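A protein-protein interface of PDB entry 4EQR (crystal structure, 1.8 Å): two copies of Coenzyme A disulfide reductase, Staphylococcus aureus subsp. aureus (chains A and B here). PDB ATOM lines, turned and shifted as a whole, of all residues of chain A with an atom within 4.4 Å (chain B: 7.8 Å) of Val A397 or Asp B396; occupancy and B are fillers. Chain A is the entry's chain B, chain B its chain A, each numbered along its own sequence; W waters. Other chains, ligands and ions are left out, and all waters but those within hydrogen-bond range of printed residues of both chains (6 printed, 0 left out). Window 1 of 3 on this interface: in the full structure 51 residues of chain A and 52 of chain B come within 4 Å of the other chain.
Among the printed residues, pairs that only touch across the chains: Lys A393 with Lys B393 (3.8 Å), Lys A393 with Asp B396 (3.4 Å), Asp A396 with Lys B393 (3.4 Å), Asp A396 with Val B397 (3.7 Å), Asp A396 with Phe B414 (3.6 Å), Val A397 with Asp B396 (3.7 Å), Val A397 with Met B400 (3.7 Å), Met A400 with Val B397 (3.6 Å), Met A400 with Met B400 (3.6 Å), Met A400 with Ala B401 (3.7 Å), Met A400 with Phe B414 (3.8 Å), Ala A401 with Met B400 (3.6 Å), Phe A414 with Asp B396 (3.6 Å), Phe A414 with Met B400 (3.8 Å), Val A416 with Asn B322 (3.4 Å), Val A416 with Asp B396 (3.4 Å) and Ala A417 with Ile B324 (3.7 Å).
Water W2 lies within hydrogen-bond range of the side-chain carboxylate of Asp A396 (2.7 Å) and the side-chain amino group of Lys B393 (2.7 Å).
Water W4 lies within hydrogen-bond range of the backbone carbonyl oxygen of Asn B322 and the backbone carbonyl oxygen of Val A416.
Water W3 lies within hydrogen-bond range of NZ of Lys A393, OD2 of Asp B396 and O of Ala A417.
Water W5 bridges the backbone NH of Glu B415 (2.8 Å) and the side-chain hydroxyl of Ser A399 (2.8 Å).
Water W6 bridges OD2 of Asp A396 and NE of Arg B394.
Water W1 bridges the side-chain carboxylate of Asp B396 (2.8 Å) and the guanidinium group of Arg A394 (3.1 Å).
The backbone carbonyl oxygen (O) of Glu B415 lies within hydrogen-bond range of the side-chain hydroxyl (OG) of Ser A399 (2.8 Å).
OD1 of Asp B392 lies within salt-bridge range of NZ of Lys A393, at 2.8 Å.
ND2 of Asn B322 sits close to N of Ala A417 (3.1 Å).
OD1 of Asp B396 lies within hydrogen-bond range of N of Ala A417 (2.8 Å).
The side-chain amide nitrogen (ND2) of Asn B322 sits at hydrogen-bond distance from the side-chain carboxylate (OD1) of Asp B396 (3.1 Å).
The side-chain amide nitrogen (ND2) of Asn B404 sits at hydrogen-bond distance from the backbone carbonyl oxygen (O) of Met B400, 3.0 Å away.
The backbone carbonyl oxygen (O) of Ser B334 sits close to the side-chain amide oxygen (OD1) of Asn B322 (3.3 Å).
Val A397 touches just these residues of chain B: Asp B396 and Met B400.
Leu A398 touches none of the printed residues of chain B.
Of the printed residues of chain B, Ala A401 touches Met B400.
Asp B396 touches just these residues of chain A: Lys A393 (3.4 Å), Val A397 (3.7 Å), Phe A414 (3.6 Å), Val A416 (3.4 Å) and Ala A417 (2.8 Å).
Asn B404 touches none of the printed residues of chain A.
Printed residues of chain A within 4 Å of Phe B414: Asp A396 and Met A400.
The nearest residue of chain B that does not touch Val A397 is Val B397 (4.04 Å).
The nearest printed residue of chain A that does not touch Asp B396 is Arg A394 (5.8 Å).
The nearest printed residue of chain B that does not touch Lys A393 is Val B397 (5.1 Å).
Of the 26 printed residues of chain B, 10 touch a printed residue of chain A.
Among the printed residues, Asp or Glu carboxylates within 4 Å of a Lys or Arg side-chain nitrogen of the other chain: Lys A393 with Asp B392 (2.8 Å).
Lys A393 touches Asp B396, and with the chains exchanged Asp A396 touches Lys B393.
Asp A396 touches Val B397, and with the chains exchanged Val A397 touches Asp B396.
Met A400 touches Ala B401, and with the chains exchanged Ala A401 touches Met B400.
Met A400 touches Phe B414, and with the chains exchanged Phe A414 touches Met B400.
Positions printed for both chains: 393, 394, 395, 396, 397, 398, 399, 400, 401, 414 and 429.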
ATOM      1  N   LYS A 393     -31.483  -5.490  13.903  1.00  0.00           N
ATOM      2  CA  LYS A 393     -30.395  -6.031  13.100  1.00  0.00           C
ATOM      3  C   LYS A 393     -30.673  -7.484  12.718  1.00  0.00           C
ATOM      4  O   LYS A 393     -30.572  -7.850  11.547  1.00  0.00           O
ATOM      5  CB  LYS A 393     -29.049  -5.905  13.828  1.00  0.00           C
ATOM      6  CG  LYS A 393     -27.881  -6.538  13.051  1.00  0.00           C
ATOM      7  CD  LYS A 393     -26.519  -6.009  13.509  1.00  0.00           C
ATOM      8  CE  LYS A 393     -26.207  -6.465  14.933  1.00  0.00           C
ATOM      9  NZ  LYS A 393     -24.852  -6.018  15.367  1.00  0.00           N
ATOM     10  N   ARG A 394     -31.021  -8.320  13.697  1.00  0.00           N
ATOM     11  CA  ARG A 394     -31.219  -9.739  13.403  1.00  0.00           C
ATOM     12  C   ARG A 394     -32.404  -9.934  12.450  1.00  0.00           C
ATOM     13  O   ARG A 394     -32.364 -10.772  11.553  1.00  0.00           O
ATOM     14  CB  ARG A 394     -31.429 -10.576  14.676  1.00  0.00           C
ATOM     15  CG  ARG A 394     -30.273 -10.592  15.686  1.00  0.00           C
ATOM     16  CD  ARG A 394     -28.938 -10.259  15.071  1.00  0.00           C
ATOM     17  NE  ARG A 394     -27.799 -10.499  15.972  1.00  0.00           N
ATOM     18  CZ  ARG A 394     -27.362  -9.644  16.896  1.00  0.00           C
ATOM     19  NH1 ARG A 394     -26.296  -9.948  17.628  1.00  0.00           N
ATOM     20  NH2 ARG A 394     -27.993  -8.496  17.113  1.00  0.00           N
ATOM     21  N   ILE A 395     -33.464  -9.161  12.637  1.00  0.00           N
ATOM     22  CA  ILE A 395     -34.638  -9.352  11.773  1.00  0.00           C
ATOM     23  C   ILE A 395     -34.419  -8.866  10.333  1.00  0.00           C
ATOM     24  O   ILE A 395     -34.861  -9.511   9.382  1.00  0.00           O
ATOM     25  CB  ILE A 395     -35.913  -8.741  12.385  1.00  0.00           C
ATOM     26  CG1 ILE A 395     -36.271  -9.491  13.665  1.00  0.00           C
ATOM     27  CG2 ILE A 395     -37.093  -8.854  11.398  1.00  0.00           C
ATOM     28  CD1 ILE A 395     -36.716 -10.939  13.414  1.00  0.00           C
ATOM     29  N   ASP A 396     -33.728  -7.744  10.162  1.00  0.00           N
ATOM     30  CA  ASP A 396     -33.351  -7.313   8.811  1.00  0.00           C
ATOM     31  C   ASP A 396     -32.431  -8.333   8.118  1.00  0.00           C
ATOM     32  O   ASP A 396     -32.541  -8.551   6.916  1.00  0.00           O
ATOM     33  CB  ASP A 396     -32.676  -5.938   8.834  1.00  0.00           C
ATOM     34  CG  ASP A 396     -33.672  -4.786   8.933  1.00  0.00           C
ATOM     35  OD1 ASP A 396     -34.890  -5.016   8.808  1.00  0.00           O
ATOM     36  OD2 ASP A 396     -33.221  -3.642   9.122  1.00  0.00           O
ATOM     37  N   VAL A 397     -31.498  -8.940   8.860  1.00  0.00           N
ATOM     38  CA  VAL A 397     -30.636  -9.951   8.245  1.00  0.00           C
ATOM     39  C   VAL A 397     -31.485 -11.134   7.782  1.00  0.00           C
ATOM     40  O   VAL A 397     -31.310 -11.652   6.675  1.00  0.00           O
ATOM     41  CB  VAL A 397     -29.522 -10.450   9.201  1.00  0.00           C
ATOM     42  CG1 VAL A 397     -28.828 -11.675   8.607  1.00  0.00           C
ATOM     43  CG2 VAL A 397     -28.518  -9.331   9.478  1.00  0.00           C
ATOM     44  N   LEU A 398     -32.427 -11.545   8.621  1.00  0.00           N
ATOM     45  CA  LEU A 398     -33.289 -12.663   8.282  1.00  0.00           C
ATOM     46  C   LEU A 398     -34.252 -12.307   7.146  1.00  0.00           C
ATOM     47  O   LEU A 398     -34.569 -13.159   6.324  1.00  0.00           O
ATOM     48  CB  LEU A 398     -34.025 -13.187   9.513  1.00  0.00           C
ATOM     49  CG  LEU A 398     -33.080 -13.885  10.509  1.00  0.00           C
ATOM     50  CD1 LEU A 398     -33.810 -14.198  11.798  1.00  0.00           C
ATOM     51  CD2 LEU A 398     -32.487 -15.152   9.904  1.00  0.00           C
ATOM     52  N   SER A 399     -34.693 -11.052   7.089  1.00  0.00           N
ATOM     53  CA  SER A 399     -35.468 -10.597   5.931  1.00  0.00           C
ATOM     54  C   SER A 399     -34.680 -10.810   4.622  1.00  0.00           C
ATOM     55  O   SER A 399     -35.213 -11.338   3.633  1.00  0.00           O
ATOM     56  CB  SER A 399     -35.888  -9.135   6.078  1.00  0.00           C
ATOM     57  OG  SER A 399     -36.656  -8.722   4.953  1.00  0.00           O
ATOM     58  N   MET A 400     -33.416 -10.403   4.626  1.00  0.00           N
ATOM     59  CA  MET A 400     -32.545 -10.588   3.466  1.00  0.00           C
ATOM     60  C   MET A 400     -32.321 -12.078   3.161  1.00  0.00           C
ATOM     61  O   MET A 400     -32.239 -12.475   1.996  1.00  0.00           O
ATOM     62  CB  MET A 400     -31.215  -9.856   3.669  1.00  0.00           C
ATOM     63  CG  MET A 400     -30.208 -10.041   2.529  1.00  0.00           C
ATOM     64  SD  MET A 400     -30.805  -9.385   0.960  1.00  0.00           S
ATOM     65  CE  MET A 400     -30.602  -7.631   1.227  1.00  0.00           C
ATOM     66  N   ALA A 401     -32.215 -12.897   4.205  1.00  0.00           N
ATOM     67  CA  ALA A 401     -32.086 -14.332   4.026  1.00  0.00           C
ATOM     68  C   ALA A 401     -33.308 -14.905   3.319  1.00  0.00           C
ATOM     69  O   ALA A 401     -33.181 -15.692   2.385  1.00  0.00           O
ATOM     70  CB  ALA A 401     -31.887 -15.030   5.377  1.00  0.00           C
ATOM     71  N   PHE A 414     -23.745 -17.641   7.785  1.00  0.00           N
ATOM     72  CA  PHE A 414     -23.847 -16.187   7.830  1.00  0.00           C
ATOM     73  C   PHE A 414     -22.609 -15.589   8.491  1.00  0.00           C
ATOM     74  O   PHE A 414     -22.289 -15.900   9.637  1.00  0.00           O
ATOM     75  CB  PHE A 414     -25.126 -15.749   8.563  1.00  0.00           C
ATOM     76  CG  PHE A 414     -25.113 -14.302   9.010  1.00  0.00           C
ATOM     77  CD1 PHE A 414     -25.017 -13.272   8.086  1.00  0.00           C
ATOM     78  CD2 PHE A 414     -25.192 -13.981  10.356  1.00  0.00           C
ATOM     79  CE1 PHE A 414     -25.004 -11.935   8.500  1.00  0.00           C
ATOM     80  CE2 PHE A 414     -25.181 -12.646  10.781  1.00  0.00           C
ATOM     81  CZ  PHE A 414     -25.091 -11.624   9.848  1.00  0.00           C
ATOM     82  N   VAL A 416     -21.114 -12.796  10.243  1.00  0.00           N
ATOM     83  CA  VAL A 416     -21.518 -11.612  11.005  1.00  0.00           C
ATOM     84  C   VAL A 416     -20.351 -10.647  11.131  1.00  0.00           C
ATOM     85  O   VAL A 416     -19.193 -11.050  11.058  1.00  0.00           O
ATOM     86  CB  VAL A 416     -22.017 -11.999  12.425  1.00  0.00           C
ATOM     87  CG1 VAL A 416     -20.840 -12.486  13.299  1.00  0.00           C
ATOM     88  CG2 VAL A 416     -22.733 -10.824  13.100  1.00  0.00           C
ATOM     89  N   ALA A 417     -20.659  -9.369  11.295  1.00  0.00           N
ATOM     90  CA  ALA A 417     -19.650  -8.396  11.651  1.00  0.00           C
ATOM     91  C   ALA A 417     -19.431  -8.511  13.157  1.00  0.00           C
ATOM     92  O   ALA A 417     -20.306  -8.124  13.938  1.00  0.00           O
ATOM     93  CB  ALA A 417     -20.122  -7.001  11.289  1.00  0.00           C
ATOM     94  N   ILE A 429     -27.859 -15.489  15.025  1.00  0.00           N
ATOM     95  CA  ILE A 429     -28.299 -16.024  13.749  1.00  0.00           C
ATOM     96  C   ILE A 429     -27.593 -17.337  13.408  1.00  0.00           C
ATOM     97  O   ILE A 429     -28.227 -18.294  12.958  1.00  0.00           O
ATOM     98  CB  ILE A 429     -28.129 -14.995  12.620  1.00  0.00           C
ATOM     99  CG1 ILE A 429     -29.163 -13.874  12.795  1.00  0.00           C
ATOM    100  CG2 ILE A 429     -28.274 -15.668  11.257  1.00  0.00           C
ATOM    101  CD1 ILE A 429     -29.012 -12.738  11.809  1.00  0.00           C
ATOM    102  N   LEU B 320     -16.260 -13.793   3.274  1.00  0.00           N
ATOM    103  CA  LEU B 320     -16.679 -12.504   2.745  1.00  0.00           C
ATOM    104  C   LEU B 320     -15.841 -11.375   3.335  1.00  0.00           C
ATOM    105  O   LEU B 320     -15.780 -10.284   2.778  1.00  0.00           O
ATOM    106  CB  LEU B 320     -18.160 -12.264   3.023  1.00  0.00           C
ATOM    107  CG  LEU B 320     -19.123 -13.165   2.250  1.00  0.00           C
ATOM    108  CD1 LEU B 320     -20.551 -12.975   2.761  1.00  0.00           C
ATOM    109  CD2 LEU B 320     -19.038 -12.831   0.777  1.00  0.00           C
ATOM    110  N   ASN B 322     -16.242  -9.942   6.525  1.00  0.00           N
ATOM    111  CA  ASN B 322     -17.021  -8.984   7.300  1.00  0.00           C
ATOM    112  C   ASN B 322     -16.225  -8.582   8.533  1.00  0.00           C
ATOM    113  O   ASN B 322     -15.694  -9.438   9.239  1.00  0.00           O
ATOM    114  CB  ASN B 322     -18.370  -9.591   7.707  1.00  0.00           C
ATOM    115  CG  ASN B 322     -19.413  -8.534   8.026  1.00  0.00           C
ATOM    116  OD1 ASN B 322     -19.101  -7.344   8.102  1.00  0.00           O
ATOM    117  ND2 ASN B 322     -20.658  -8.970   8.236  1.00  0.00           N
ATOM    118  N   ASN B 323     -16.105  -7.283   8.769  1.00  0.00           N
ATOM    119  CA  ASN B 323     -15.283  -6.790   9.875  1.00  0.00           C
ATOM    120  C   ASN B 323     -15.800  -5.473  10.424  1.00  0.00           C
ATOM    121  O   ASN B 323     -16.480  -4.712   9.727  1.00  0.00           O
ATOM    122  CB  ASN B 323     -13.831  -6.615   9.433  1.00  0.00           C
ATOM    123  CG  ASN B 323     -13.669  -5.477   8.442  1.00  0.00           C
ATOM    124  OD1 ASN B 323     -13.376  -4.354   8.831  1.00  0.00           O
ATOM    125  ND2 ASN B 323     -13.899  -5.757   7.160  1.00  0.00           N
ATOM    126  N   ILE B 324     -15.474  -5.193  11.679  1.00  0.00           N
ATOM    127  CA  ILE B 324     -16.044  -4.022  12.325  1.00  0.00           C
ATOM    128  C   ILE B 324     -15.223  -3.609  13.536  1.00  0.00           C
ATOM    129  O   ILE B 324     -14.578  -4.437  14.191  1.00  0.00           O
ATOM    130  CB  ILE B 324     -17.512  -4.306  12.759  1.00  0.00           C
ATOM    131  CG1 ILE B 324     -18.206  -3.036  13.251  1.00  0.00           C
ATOM    132  CG2 ILE B 324     -17.563  -5.385  13.851  1.00  0.00           C
ATOM    133  CD1 ILE B 324     -19.711  -3.205  13.291  1.00  0.00           C
ATOM    134  N   ALA B 333     -17.500  -0.346   9.656  1.00  0.00           N
ATOM    135  CA  ALA B 333     -17.693  -1.728   9.209  1.00  0.00           C
ATOM    136  C   ALA B 333     -17.579  -1.869   7.693  1.00  0.00           C
ATOM    137  O   ALA B 333     -18.006  -0.989   6.948  1.00  0.00           O
ATOM    138  CB  ALA B 333     -19.037  -2.266   9.684  1.00  0.00           C
ATOM    139  N   SER B 334     -16.982  -2.974   7.252  1.00  0.00           N
ATOM    140  CA  SER B 334     -16.926  -3.290   5.832  1.00  0.00           C
ATOM    141  C   SER B 334     -17.004  -4.783   5.586  1.00  0.00           C
ATOM    142  O   SER B 334     -16.797  -5.594   6.486  1.00  0.00           O
ATOM    143  CB  SER B 334     -15.685  -2.698   5.158  1.00  0.00           C
ATOM    144  OG  SER B 334     -14.479  -3.265   5.655  1.00  0.00           O
ATOM    145  N   VAL B 335     -17.328  -5.140   4.351  1.00  0.00           N
ATOM    146  CA  VAL B 335     -17.403  -6.538   3.979  1.00  0.00           C
ATOM    147  C   VAL B 335     -17.080  -6.660   2.492  1.00  0.00           C
ATOM    148  O   VAL B 335     -17.327  -5.727   1.719  1.00  0.00           O
ATOM    149  CB  VAL B 335     -18.800  -7.123   4.311  1.00  0.00           C
ATOM    150  CG1 VAL B 335     -19.919  -6.359   3.573  1.00  0.00           C
ATOM    151  CG2 VAL B 335     -18.856  -8.605   4.013  1.00  0.00           C
ATOM    152  N   ALA B 385     -19.597   0.925   5.772  1.00  0.00           N
ATOM    153  CA  ALA B 385     -20.498   1.859   6.440  1.00  0.00           C
ATOM    154  C   ALA B 385     -19.804   2.486   7.630  1.00  0.00           C
ATOM    155  O   ALA B 385     -19.063   1.824   8.359  1.00  0.00           O
ATOM    156  CB  ALA B 385     -21.791   1.158   6.878  1.00  0.00           C
ATOM    157  N   GLY B 390     -26.201   2.434  13.382  1.00  0.00           N
ATOM    158  CA  GLY B 390     -26.767   1.714  12.261  1.00  0.00           C
ATOM    159  C   GLY B 390     -25.806   1.111  11.253  1.00  0.00           C
ATOM    160  O   GLY B 390     -26.247   0.389  10.376  1.00  0.00           O
ATOM    161  N   ALA B 391     -24.508   1.388  11.365  1.00  0.00           N
ATOM    162  CA  ALA B 391     -23.558   0.828  10.398  1.00  0.00           C
ATOM    163  C   ALA B 391     -23.446  -0.698  10.490  1.00  0.00           C
ATOM    164  O   ALA B 391     -23.329  -1.377   9.476  1.00  0.00           O
ATOM    165  CB  ALA B 391     -22.173   1.489  10.526  1.00  0.00           C
ATOM    166  N   ASP B 392     -23.464  -1.238  11.704  1.00  0.00           N
ATOM    167  CA  ASP B 392     -23.415  -2.683  11.863  1.00  0.00           C
ATOM    168  C   ASP B 392     -24.616  -3.374  11.210  1.00  0.00           C
ATOM    169  O   ASP B 392     -24.473  -4.408  10.543  1.00  0.00           O
ATOM    170  CB  ASP B 392     -23.280  -3.085  13.340  1.00  0.00           C
ATOM    171  CG  ASP B 392     -24.394  -2.519  14.211  1.00  0.00           C
ATOM    172  OD1 ASP B 392     -24.824  -3.222  15.143  1.00  0.00           O
ATOM    173  OD2 ASP B 392     -24.852  -1.390  13.953  1.00  0.00           O
ATOM    174  N   LYS B 393     -25.800  -2.813  11.407  1.00  0.00           N
ATOM    175  CA  LYS B 393     -26.996  -3.389  10.804  1.00  0.00           C
ATOM    176  C   LYS B 393     -26.901  -3.415   9.264  1.00  0.00           C
ATOM    177  O   LYS B 393     -27.159  -4.452   8.640  1.00  0.00           O
ATOM    178  CB  LYS B 393     -28.270  -2.648  11.273  1.00  0.00           C
ATOM    179  CG  LYS B 393     -29.554  -3.124  10.558  1.00  0.00           C
ATOM    180  CD  LYS B 393     -30.788  -2.673  11.317  1.00  0.00           C
ATOM    181  CE  LYS B 393     -30.968  -1.164  11.220  1.00  0.00           C
ATOM    182  NZ  LYS B 393     -32.233  -0.722  11.883  1.00  0.00           N
ATOM    183  N   ARG B 394     -26.517  -2.295   8.650  1.00  0.00           N
ATOM    184  CA  ARG B 394     -26.468  -2.245   7.188  1.00  0.00           C
ATOM    185  C   ARG B 394     -25.435  -3.234   6.631  1.00  0.00           C
ATOM    186  O   ARG B 394     -25.679  -3.903   5.629  1.00  0.00           O
ATOM    187  CB  ARG B 394     -26.190  -0.829   6.647  1.00  0.00           C
ATOM    188  CG  ARG B 394     -27.213   0.252   7.020  1.00  0.00           C
ATOM    189  CD  ARG B 394     -28.606  -0.335   7.283  1.00  0.00           C
ATOM    190  NE  ARG B 394     -29.669   0.677   7.379  1.00  0.00           N
ATOM    191  CZ  ARG B 394     -29.922   1.406   8.462  1.00  0.00           C
ATOM    192  NH1 ARG B 394     -30.926   2.285   8.460  1.00  0.00           N
ATOM    193  NH2 ARG B 394     -29.169   1.274   9.541  1.00  0.00           N
ATOM    194  N   ILE B 395     -24.276  -3.328   7.281  1.00  0.00           N
ATOM    195  CA  ILE B 395     -23.226  -4.198   6.765  1.00  0.00           C
ATOM    196  C   ILE B 395     -23.569  -5.681   6.952  1.00  0.00           C
ATOM    197  O   ILE B 395     -23.273  -6.492   6.086  1.00  0.00           O
ATOM    198  CB  ILE B 395     -21.826  -3.828   7.336  1.00  0.00           C
ATOM    199  CG1 ILE B 395     -21.394  -2.453   6.814  1.00  0.00           C
ATOM    200  CG2 ILE B 395     -20.773  -4.878   6.949  1.00  0.00           C
ATOM    201  CD1 ILE B 395     -21.300  -2.360   5.266  1.00  0.00           C
ATOM    202  N   ASP B 396     -24.220  -6.034   8.055  1.00  0.00           N
ATOM    203  CA  ASP B 396     -24.675  -7.417   8.219  1.00  0.00           C
ATOM    204  C   ASP B 396     -25.708  -7.796   7.160  1.00  0.00           C
ATOM    205  O   ASP B 396     -25.695  -8.913   6.646  1.00  0.00           O
ATOM    206  CB  ASP B 396     -25.236  -7.678   9.622  1.00  0.00           C
ATOM    207  CG  ASP B 396     -24.141  -8.065  10.637  1.00  0.00           C
ATOM    208  OD1 ASP B 396     -22.972  -8.255  10.228  1.00  0.00           O
ATOM    209  OD2 ASP B 396     -24.468  -8.184  11.836  1.00  0.00           O
ATOM    210  N   VAL B 397     -26.622  -6.881   6.846  1.00  0.00           N
ATOM    211  CA  VAL B 397     -27.596  -7.174   5.799  1.00  0.00           C
ATOM    212  C   VAL B 397     -26.871  -7.397   4.473  1.00  0.00           C
ATOM    213  O   VAL B 397     -27.195  -8.310   3.717  1.00  0.00           O
ATOM    214  CB  VAL B 397     -28.662  -6.057   5.663  1.00  0.00           C
ATOM    215  CG1 VAL B 397     -29.516  -6.273   4.413  1.00  0.00           C
ATOM    216  CG2 VAL B 397     -29.521  -6.009   6.915  1.00  0.00           C
ATOM    217  N   LEU B 398     -25.871  -6.579   4.198  1.00  0.00           N
ATOM    218  CA  LEU B 398     -25.156  -6.702   2.938  1.00  0.00           C
ATOM    219  C   LEU B 398     -24.274  -7.957   2.910  1.00  0.00           C
ATOM    220  O   LEU B 398     -24.068  -8.557   1.861  1.00  0.00           O
ATOM    221  CB  LEU B 398     -24.374  -5.422   2.651  1.00  0.00           C
ATOM    222  CG  LEU B 398     -25.341  -4.283   2.266  1.00  0.00           C
ATOM    223  CD1 LEU B 398     -24.643  -2.943   2.251  1.00  0.00           C
ATOM    224  CD2 LEU B 398     -25.974  -4.577   0.914  1.00  0.00           C
ATOM    225  N   SER B 399     -23.768  -8.371   4.068  1.00  0.00           N
ATOM    226  CA  SER B 399     -23.066  -9.655   4.128  1.00  0.00           C
ATOM    227  C   SER B 399     -24.008 -10.792   3.699  1.00  0.00           C
ATOM    228  O   SER B 399     -23.628 -11.670   2.917  1.00  0.00           O
ATOM    229  CB  SER B 399     -22.531  -9.918   5.541  1.00  0.00           C
ATOM    230  OG  SER B 399     -21.884 -11.173   5.585  1.00  0.00           O
ATOM    231  N   MET B 400     -25.242 -10.769   4.207  1.00  0.00           N
ATOM    232  CA  MET B 400     -26.217 -11.794   3.865  1.00  0.00           C
ATOM    233  C   MET B 400     -26.584 -11.738   2.377  1.00  0.00           C
ATOM    234  O   MET B 400     -26.786 -12.775   1.743  1.00  0.00           O
ATOM    235  CB  MET B 400     -27.470 -11.677   4.745  1.00  0.00           C
ATOM    236  CG  MET B 400     -28.599 -12.654   4.369  1.00  0.00           C
ATOM    237  SD  MET B 400     -28.154 -14.406   4.505  1.00  0.00           S
ATOM    238  CE  MET B 400     -28.055 -14.582   6.285  1.00  0.00           C
ATOM    239  N   ALA B 401     -26.654 -10.530   1.824  1.00  0.00           N
ATOM    240  CA  ALA B 401     -26.925 -10.370   0.398  1.00  0.00           C
ATOM    241  C   ALA B 401     -25.783 -10.960  -0.434  1.00  0.00           C
ATOM    242  O   ALA B 401     -26.022 -11.698  -1.385  1.00  0.00           O
ATOM    243  CB  ALA B 401     -27.136  -8.892   0.052  1.00  0.00           C
ATOM    244  N   MET B 402     -24.547 -10.642  -0.058  1.00  0.00           N
ATOM    245  CA  MET B 402     -23.372 -11.089  -0.807  1.00  0.00           C
ATOM    246  C   MET B 402     -23.212 -12.601  -0.741  1.00  0.00           C
ATOM    247  O   MET B 402     -22.816 -13.247  -1.713  1.00  0.00           O
ATOM    248  CB  MET B 402     -22.120 -10.400  -0.268  1.00  0.00           C
ATOM    249  CG  MET B 402     -22.090  -8.940  -0.613  1.00  0.00           C
ATOM    250  SD  MET B 402     -20.894  -8.039   0.367  1.00  0.00           S
ATOM    251  CE  MET B 402     -19.414  -8.465  -0.514  1.00  0.00           C
ATOM    252  N   MET B 403     -23.537 -13.158   0.418  1.00  0.00           N
ATOM    253  CA  MET B 403     -23.514 -14.600   0.620  1.00  0.00           C
ATOM    254  C   MET B 403     -24.342 -15.268  -0.461  1.00  0.00           C
ATOM    255  O   MET B 403     -24.147 -16.431  -0.804  1.00  0.00           O
ATOM    256  CB  MET B 403     -24.089 -14.909   1.999  1.00  0.00           C
ATOM    257  CG  MET B 403     -24.404 -16.351   2.268  1.00  0.00           C
ATOM    258  SD  MET B 403     -25.036 -16.499   3.954  1.00  0.00           S
ATOM    259  CE  MET B 403     -25.693 -18.163   3.884  1.00  0.00           C
ATOM    260  N   ASN B 404     -25.263 -14.502  -1.015  1.00  0.00           N
ATOM    261  CA  ASN B 404     -26.128 -15.008  -2.060  1.00  0.00           C
ATOM    262  C   ASN B 404     -25.831 -14.370  -3.418  1.00  0.00           C
ATOM    263  O   ASN B 404     -26.649 -14.426  -4.331  1.00  0.00           O
ATOM    264  CB  ASN B 404     -27.581 -14.805  -1.645  1.00  0.00           C
ATOM    265  CG  ASN B 404     -27.965 -15.680  -0.473  1.00  0.00           C
ATOM    266  OD1 ASN B 404     -27.875 -16.903  -0.554  1.00  0.00           O
ATOM    267  ND2 ASN B 404     -28.379 -15.061   0.630  1.00  0.00           N
ATOM    268  N   PHE B 414     -35.164  -5.124  -0.959  1.00  0.00           N
ATOM    269  CA  PHE B 414     -34.935  -5.451   0.441  1.00  0.00           C
ATOM    270  C   PHE B 414     -36.046  -4.874   1.308  1.00  0.00           C
ATOM    271  O   PHE B 414     -36.321  -3.684   1.249  1.00  0.00           O
ATOM    272  CB  PHE B 414     -33.580  -4.900   0.895  1.00  0.00           C
ATOM    273  CG  PHE B 414     -33.398  -4.881   2.389  1.00  0.00           C
ATOM    274  CD1 PHE B 414     -33.463  -6.054   3.124  1.00  0.00           C
ATOM    275  CD2 PHE B 414     -33.138  -3.687   3.053  1.00  0.00           C
ATOM    276  CE1 PHE B 414     -33.268  -6.045   4.497  1.00  0.00           C
ATOM    277  CE2 PHE B 414     -32.949  -3.663   4.435  1.00  0.00           C
ATOM    278  CZ  PHE B 414     -33.023  -4.837   5.155  1.00  0.00           C
ATOM    279  N   GLU B 415     -36.689  -5.722   2.104  1.00  0.00           N
ATOM    280  CA  GLU B 415     -37.806  -5.279   2.922  1.00  0.00           C
ATOM    281  C   GLU B 415     -37.321  -5.025   4.350  1.00  0.00           C
ATOM    282  O   GLU B 415     -37.205  -5.946   5.153  1.00  0.00           O
ATOM    283  CB  GLU B 415     -38.949  -6.309   2.894  1.00  0.00           C
ATOM    284  CG  GLU B 415     -40.239  -5.815   3.551  1.00  0.00           C
ATOM    285  CD  GLU B 415     -41.413  -6.765   3.375  1.00  0.00           C
ATOM    286  OE1 GLU B 415     -42.233  -6.860   4.315  1.00  0.00           O
ATOM    287  OE2 GLU B 415     -41.516  -7.424   2.316  1.00  0.00           O
ATOM    288  N   ILE B 429     -30.262   1.045   2.409  1.00  0.00           N
ATOM    289  CA  ILE B 429     -29.981  -0.098   1.548  1.00  0.00           C
ATOM    290  C   ILE B 429     -30.801  -0.025   0.254  1.00  0.00           C
ATOM    291  O   ILE B 429     -30.271  -0.201  -0.860  1.00  0.00           O
ATOM    292  CB  ILE B 429     -30.177  -1.440   2.302  1.00  0.00           C
ATOM    293  CG1 ILE B 429     -29.001  -1.653   3.269  1.00  0.00           C
ATOM    294  CG2 ILE B 429     -30.229  -2.608   1.324  1.00  0.00           C
ATOM    295  CD1 ILE B 429     -29.156  -2.816   4.199  1.00  0.00           C
HETATM  296  O   HOH W   1     -26.310  -9.740  13.319  1.00  0.00           O
HETATM  297  O   HOH W   2     -34.400  -1.806  10.700  1.00  0.00           O
HETATM  298  O   HOH W   3     -22.922  -7.149  13.823  1.00  0.00           O
HETATM  299  O   HOH W   4     -16.546 -10.495  11.567  1.00  0.00           O
HETATM  300  O   HOH W   5     -35.883  -8.351   2.248  1.00  0.00           O
HETATM  301  O   HOH W   6     -31.347  -2.097   7.677  1.00  0.00           O
